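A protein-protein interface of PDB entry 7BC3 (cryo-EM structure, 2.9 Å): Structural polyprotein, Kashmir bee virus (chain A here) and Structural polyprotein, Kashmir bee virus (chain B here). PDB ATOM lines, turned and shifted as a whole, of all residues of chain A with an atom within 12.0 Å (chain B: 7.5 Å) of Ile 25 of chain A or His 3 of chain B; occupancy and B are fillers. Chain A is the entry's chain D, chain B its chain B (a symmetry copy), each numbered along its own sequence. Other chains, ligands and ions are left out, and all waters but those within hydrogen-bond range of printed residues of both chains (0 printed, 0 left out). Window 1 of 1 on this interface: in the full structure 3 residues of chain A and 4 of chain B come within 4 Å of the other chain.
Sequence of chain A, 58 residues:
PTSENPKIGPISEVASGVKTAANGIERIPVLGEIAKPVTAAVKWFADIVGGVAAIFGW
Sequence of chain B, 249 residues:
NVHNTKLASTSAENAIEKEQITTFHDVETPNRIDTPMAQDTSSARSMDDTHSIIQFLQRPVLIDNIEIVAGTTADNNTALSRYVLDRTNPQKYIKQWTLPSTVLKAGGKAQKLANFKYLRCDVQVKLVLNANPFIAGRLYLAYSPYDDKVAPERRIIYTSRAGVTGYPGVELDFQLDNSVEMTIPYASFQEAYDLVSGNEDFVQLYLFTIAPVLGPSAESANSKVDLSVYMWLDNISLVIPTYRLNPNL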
ATOM      1  N   VAL A  18      23.968 -14.065 -10.038  1.00  0.00           N
ATOM      2  CA  VAL A  18      22.880 -13.183  -9.637  1.00  0.00           C
ATOM      3  C   VAL A  18      22.886 -11.963 -10.549  1.00  0.00           C
ATOM      4  O   VAL A  18      23.951 -11.442 -10.898  1.00  0.00           O
ATOM      5  CB  VAL A  18      23.010 -12.768  -8.155  1.00  0.00           C
ATOM      6  CG1 VAL A  18      21.946 -11.755  -7.774  1.00  0.00           C
ATOM      7  CG2 VAL A  18      22.919 -13.988  -7.251  1.00  0.00           C
ATOM      8  N   LYS A  19      21.693 -11.509 -10.932  1.00  0.00           N
ATOM      9  CA  LYS A  19      21.501 -10.388 -11.848  1.00  0.00           C
ATOM     10  C   LYS A  19      20.717  -9.265 -11.178  1.00  0.00           C
ATOM     11  O   LYS A  19      19.810  -8.677 -11.773  1.00  0.00           O
ATOM     12  CB  LYS A  19      20.770 -10.830 -13.116  1.00  0.00           C
ATOM     13  CG  LYS A  19      21.620 -11.462 -14.206  1.00  0.00           C
ATOM     14  CD  LYS A  19      22.057 -12.875 -13.854  1.00  0.00           C
ATOM     15  CE  LYS A  19      22.845 -13.520 -14.996  1.00  0.00           C
ATOM     16  NZ  LYS A  19      23.083 -14.740 -14.174  1.00  0.00           N
ATOM     17  N   THR A  20      21.054  -8.944  -9.931  1.00  0.00           N
ATOM     18  CA  THR A  20      20.271  -7.990  -9.159  1.00  0.00           C
ATOM     19  C   THR A  20      21.179  -7.189  -8.239  1.00  0.00           C
ATOM     20  O   THR A  20      22.154  -7.719  -7.698  1.00  0.00           O
ATOM     21  CB  THR A  20      19.206  -8.695  -8.310  1.00  0.00           C
ATOM     22  OG1 THR A  20      19.849  -9.534  -7.345  1.00  0.00           O
ATOM     23  CG2 THR A  20      18.294  -9.553  -9.174  1.00  0.00           C
ATOM     24  N   ALA A  21      20.848  -5.913  -8.064  1.00  0.00           N
ATOM     25  CA  ALA A  21      21.497  -5.111  -7.039  1.00  0.00           C
ATOM     26  C   ALA A  21      21.228  -5.731  -5.677  1.00  0.00           C
ATOM     27  O   ALA A  21      20.085  -5.757  -5.209  1.00  0.00           O
ATOM     28  CB  ALA A  21      20.988  -3.673  -7.090  1.00  0.00           C
ATOM     29  N   ALA A  22      22.286  -6.237  -5.041  1.00  0.00           N
ATOM     30  CA  ALA A  22      22.118  -7.012  -3.819  1.00  0.00           C
ATOM     31  C   ALA A  22      21.439  -6.217  -2.713  1.00  0.00           C
ATOM     32  O   ALA A  22      20.736  -6.806  -1.886  1.00  0.00           O
ATOM     33  CB  ALA A  22      23.473  -7.523  -3.339  1.00  0.00           C
ATOM     34  N   ASN A  23      21.631  -4.901  -2.675  1.00  0.00           N
ATOM     35  CA  ASN A  23      20.972  -4.046  -1.700  1.00  0.00           C
ATOM     36  C   ASN A  23      19.645  -3.505  -2.211  1.00  0.00           C
ATOM     37  O   ASN A  23      19.089  -2.582  -1.609  1.00  0.00           O
ATOM     38  CB  ASN A  23      21.891  -2.889  -1.309  1.00  0.00           C
ATOM     39  CG  ASN A  23      22.059  -1.879  -2.421  1.00  0.00           C
ATOM     40  OD1 ASN A  23      22.319  -2.237  -3.570  1.00  0.00           O
ATOM     41  ND2 ASN A  23      21.915  -0.604  -2.085  1.00  0.00           N
ATOM     42  N   GLY A  24      19.126  -4.060  -3.307  1.00  0.00           N
ATOM     43  CA  GLY A  24      17.868  -3.620  -3.863  1.00  0.00           C
ATOM     44  C   GLY A  24      16.682  -4.363  -3.278  1.00  0.00           C
ATOM     45  O   GLY A  24      16.814  -5.356  -2.564  1.00  0.00           O
ATOM     46  N   ILE A  25      15.491  -3.861  -3.612  1.00  0.00           N
ATOM     47  CA  ILE A  25      14.252  -4.403  -3.063  1.00  0.00           C
ATOM     48  C   ILE A  25      13.736  -5.600  -3.847  1.00  0.00           C
ATOM     49  O   ILE A  25      12.881  -6.339  -3.336  1.00  0.00           O
ATOM     50  CB  ILE A  25      13.175  -3.299  -3.009  1.00  0.00           C
ATOM     51  CG1 ILE A  25      11.888  -3.828  -2.380  1.00  0.00           C
ATOM     52  CG2 ILE A  25      12.901  -2.744  -4.399  1.00  0.00           C
ATOM     53  CD1 ILE A  25      11.000  -2.738  -1.839  1.00  0.00           C
ATOM     54  N   GLU A  26      14.228  -5.821  -5.061  1.00  0.00           N
ATOM     55  CA  GLU A  26      13.797  -6.968  -5.844  1.00  0.00           C
ATOM     56  C   GLU A  26      14.260  -8.266  -5.196  1.00  0.00           C
ATOM     57  O   GLU A  26      15.343  -8.336  -4.607  1.00  0.00           O
ATOM     58  CB  GLU A  26      14.341  -6.874  -7.267  1.00  0.00           C
ATOM     59  CG  GLU A  26      14.042  -5.559  -7.956  1.00  0.00           C
ATOM     60  CD  GLU A  26      14.041  -5.678  -9.467  1.00  0.00           C
ATOM     61  OE1 GLU A  26      14.976  -5.152 -10.109  1.00  0.00           O
ATOM     62  OE2 GLU A  26      13.109  -6.303 -10.015  1.00  0.00           O
ATOM     63  N   ARG A  27      13.425  -9.296  -5.303  1.00  0.00           N
ATOM     64  CA  ARG A  27      13.759 -10.602  -4.757  1.00  0.00           C
ATOM     65  C   ARG A  27      15.104 -11.084  -5.284  1.00  0.00           C
ATOM     66  O   ARG A  27      15.529 -10.729  -6.387  1.00  0.00           O
ATOM     67  CB  ARG A  27      12.672 -11.615  -5.114  1.00  0.00           C
ATOM     68  CG  ARG A  27      11.341 -11.341  -4.455  1.00  0.00           C
ATOM     69  CD  ARG A  27      10.211 -12.060  -5.164  1.00  0.00           C
ATOM     70  NE  ARG A  27       8.905 -11.588  -4.716  1.00  0.00           N
ATOM     71  CZ  ARG A  27       7.755 -11.907  -5.298  1.00  0.00           C
ATOM     72  NH1 ARG A  27       6.617 -11.426  -4.819  1.00  0.00           N
ATOM     73  NH2 ARG A  27       7.739 -12.708  -6.356  1.00  0.00           N
ATOM     74  N   ILE A  28      15.773 -11.903  -4.483  1.00  0.00           N
ATOM     75  CA  ILE A  28      17.010 -12.568  -4.866  1.00  0.00           C
ATOM     76  C   ILE A  28      16.814 -14.064  -4.656  1.00  0.00           C
ATOM     77  O   ILE A  28      16.588 -14.502  -3.524  1.00  0.00           O
ATOM     78  CB  ILE A  28      18.218 -12.069  -4.058  1.00  0.00           C
ATOM     79  CG1 ILE A  28      18.619 -10.668  -4.501  1.00  0.00           C
ATOM     80  CG2 ILE A  28      19.397 -12.998  -4.252  1.00  0.00           C
ATOM     81  CD1 ILE A  28      19.469  -9.929  -3.500  1.00  0.00           C
ATOM     82  N   PRO A  29      16.884 -14.891  -5.699  1.00  0.00           N
ATOM     83  CA  PRO A  29      16.864 -16.342  -5.478  1.00  0.00           C
ATOM     84  C   PRO A  29      18.077 -16.781  -4.675  1.00  0.00           C
ATOM     85  O   PRO A  29      19.223 -16.560  -5.074  1.00  0.00           O
ATOM     86  CB  PRO A  29      16.880 -16.915  -6.900  1.00  0.00           C
ATOM     87  CG  PRO A  29      16.369 -15.819  -7.757  1.00  0.00           C
ATOM     88  CD  PRO A  29      16.869 -14.561  -7.132  1.00  0.00           C
ATOM     89  N   GLU A  33      22.672 -17.741  -5.187  1.00  0.00           N
ATOM     90  CA  GLU A  33      23.740 -17.130  -4.407  1.00  0.00           C
ATOM     91  C   GLU A  33      24.935 -18.064  -4.269  1.00  0.00           C
ATOM     92  O   GLU A  33      26.063 -17.595  -4.078  1.00  0.00           O
ATOM     93  CB  GLU A  33      23.210 -16.729  -3.032  1.00  0.00           C
ATOM     94  CG  GLU A  33      22.071 -15.732  -3.081  1.00  0.00           C
ATOM     95  CD  GLU A  33      21.670 -15.239  -1.708  1.00  0.00           C
ATOM     96  OE1 GLU A  33      22.193 -15.769  -0.708  1.00  0.00           O
ATOM     97  OE2 GLU A  33      20.828 -14.321  -1.633  1.00  0.00           O
ATOM     98  N   ASN B   1       5.880  -5.244  -5.572  1.00  0.00           N
ATOM     99  CA  ASN B   1       6.917  -4.276  -5.233  1.00  0.00           C
ATOM    100  C   ASN B   1       7.366  -4.431  -3.788  1.00  0.00           C
ATOM    101  O   ASN B   1       8.557  -4.368  -3.488  1.00  0.00           O
ATOM    102  CB  ASN B   1       6.421  -2.851  -5.470  1.00  0.00           C
ATOM    103  CG  ASN B   1       5.047  -2.598  -4.892  1.00  0.00           C
ATOM    104  OD1 ASN B   1       4.401  -3.489  -4.339  1.00  0.00           O
ATOM    105  ND2 ASN B   1       4.593  -1.365  -5.033  1.00  0.00           N
ATOM    106  N   VAL B   2       6.403  -4.635  -2.898  1.00  0.00           N
ATOM    107  CA  VAL B   2       6.676  -4.774  -1.485  1.00  0.00           C
ATOM    108  C   VAL B   2       6.583  -6.248  -1.105  1.00  0.00           C
ATOM    109  O   VAL B   2       6.130  -7.085  -1.881  1.00  0.00           O
ATOM    110  CB  VAL B   2       5.724  -3.908  -0.628  1.00  0.00           C
ATOM    111  CG1 VAL B   2       5.978  -2.437  -0.893  1.00  0.00           C
ATOM    112  CG2 VAL B   2       4.274  -4.270  -0.900  1.00  0.00           C
ATOM    113  N   HIS B   3       7.013  -6.567   0.111  1.00  0.00           N
ATOM    114  CA  HIS B   3       7.172  -7.943   0.552  1.00  0.00           C
ATOM    115  C   HIS B   3       6.315  -8.215   1.778  1.00  0.00           C
ATOM    116  O   HIS B   3       6.088  -7.331   2.610  1.00  0.00           O
ATOM    117  CB  HIS B   3       8.638  -8.237   0.868  1.00  0.00           C
ATOM    118  CG  HIS B   3       9.571  -7.899  -0.251  1.00  0.00           C
ATOM    119  ND1 HIS B   3       9.413  -8.400  -1.524  1.00  0.00           N
ATOM    120  CD2 HIS B   3      10.663  -7.103  -0.292  1.00  0.00           C
ATOM    121  CE1 HIS B   3      10.373  -7.932  -2.301  1.00  0.00           C
ATOM    122  NE2 HIS B   3      11.145  -7.142  -1.578  1.00  0.00           N
ATOM    123  N   ASN B   4       5.836  -9.454   1.875  1.00  0.00           N
ATOM    124  CA  ASN B   4       5.054  -9.976   2.991  1.00  0.00           C
ATOM    125  C   ASN B   4       3.704  -9.293   3.146  1.00  0.00           C
ATOM    126  O   ASN B   4       2.977  -9.611   4.094  1.00  0.00           O
ATOM    127  CB  ASN B   4       5.798  -9.857   4.327  1.00  0.00           C
ATOM    128  CG  ASN B   4       6.583 -11.098   4.672  1.00  0.00           C
ATOM    129  OD1 ASN B   4       6.857 -11.937   3.815  1.00  0.00           O
ATOM    130  ND2 ASN B   4       6.946 -11.224   5.939  1.00  0.00           N
ATOM    131  N   THR B   5       3.334  -8.379   2.254  1.00  0.00           N
ATOM    132  CA  THR B   5       2.154  -7.554   2.458  1.00  0.00           C
ATOM    133  C   THR B   5       1.324  -7.492   1.188  1.00  0.00           C
ATOM    134  O   THR B   5       1.851  -7.215   0.107  1.00  0.00           O
ATOM    135  CB  THR B   5       2.546  -6.136   2.891  1.00  0.00           C
ATOM    136  OG1 THR B   5       3.418  -6.203   4.026  1.00  0.00           O
ATOM    137  CG2 THR B   5       1.316  -5.324   3.250  1.00  0.00           C
ATOM    138  N   LYS B   6       0.031  -7.755   1.334  1.00  0.00           N
ATOM    139  CA  LYS B   6      -0.964  -7.446   0.319  1.00  0.00           C
ATOM    140  C   LYS B   6      -1.529  -6.066   0.617  1.00  0.00           C
ATOM    141  O   LYS B   6      -1.937  -5.790   1.750  1.00  0.00           O
ATOM    142  CB  LYS B   6      -2.086  -8.484   0.318  1.00  0.00           C
ATOM    143  CG  LYS B   6      -2.886  -8.485   1.618  1.00  0.00           C
ATOM    144  CD  LYS B   6      -3.940  -9.562   1.688  1.00  0.00           C
ATOM    145  CE  LYS B   6      -4.675  -9.451   3.003  1.00  0.00           C
ATOM    146  NZ  LYS B   6      -3.767  -9.688   4.153  1.00  0.00           N
ATOM    147  N   ILE B  33      -2.412 -12.846  -1.101  1.00  0.00           N
ATOM    148  CA  ILE B  33      -1.050 -12.937  -0.589  1.00  0.00           C
ATOM    149  C   ILE B  33      -0.658 -14.407  -0.647  1.00  0.00           C
ATOM    150  O   ILE B  33      -1.086 -15.216   0.184  1.00  0.00           O
ATOM    151  CB  ILE B  33      -0.918 -12.365   0.828  1.00  0.00           C
ATOM    152  CG1 ILE B  33       0.540 -12.384   1.287  1.00  0.00           C
ATOM    153  CG2 ILE B  33      -1.753 -13.148   1.822  1.00  0.00           C
ATOM    154  CD1 ILE B  33       1.419 -11.396   0.578  1.00  0.00           C
ATOM    155  N   PRO B  36       6.131 -16.201  -2.050  1.00  0.00           N
ATOM    156  CA  PRO B  36       7.076 -16.034  -3.153  1.00  0.00           C
ATOM    157  C   PRO B  36       8.054 -17.199  -3.338  1.00  0.00           C
ATOM    158  O   PRO B  36       8.684 -17.589  -2.368  1.00  0.00           O
ATOM    159  CB  PRO B  36       7.850 -14.742  -2.844  1.00  0.00           C
ATOM    160  CG  PRO B  36       7.781 -14.625  -1.345  1.00  0.00           C
ATOM    161  CD  PRO B  36       6.426 -15.197  -0.993  1.00  0.00           C
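O of Ile 25 of chain A is in hydrogen-bond range of NE2 of His 3 of chain B.
Ile 25 of chain A touches Asn 1 of chain B.
Arg 27 of chain A touches Pro 36 of chain B (CZ to CB, 3.8 Å).
Thr 20 of chain A touches none of the printed residues of chain B.
Ile 25 of chain A touches just these residues of chain B: Asn 1 and His 3.
Printed residues of chain B within 4 Å of Arg 27 of chain A: Pro 36 (3.8 Å).
No residue of chain A comes within 4 Å of Val 2 of chain B.
Of the printed residues of chain A, His 3 of chain B touches Ile 25 (2.6 Å).
No residue of chain A comes within 4 Å of Thr 5 of chain B.
Of the printed residues of chain A, Pro 36 of chain B touches Arg 27.
The nearest residue of chain A that does not touch His 3 of chain B is Arg 27 of chain A (4.1 Å).
O of His 3 of chain B lies within hydrogen-bond range of OG1 of Thr 5 of chain B.
Hydrophobic or aromatic side chains of chain A that line the printed part of chain B: Ile 25.
Of the 8 printed residues of chain B, 3 touch a printed residue of chain A.
Printed residues of chain B that touch a printed residue of chain A: Asn 1, His 3 and Pro 36.
Hydrophobic or aromatic side chains of chain B within 4 Å of the printed part of chain A: His 3 and Pro 36.
Among the printed residues, 3 pairs touch across the chains.
Among the printed residues, no Asp or Glu carboxylate lies within 4 Å of a Lys or Arg side-chain nitrogen of the other chain.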
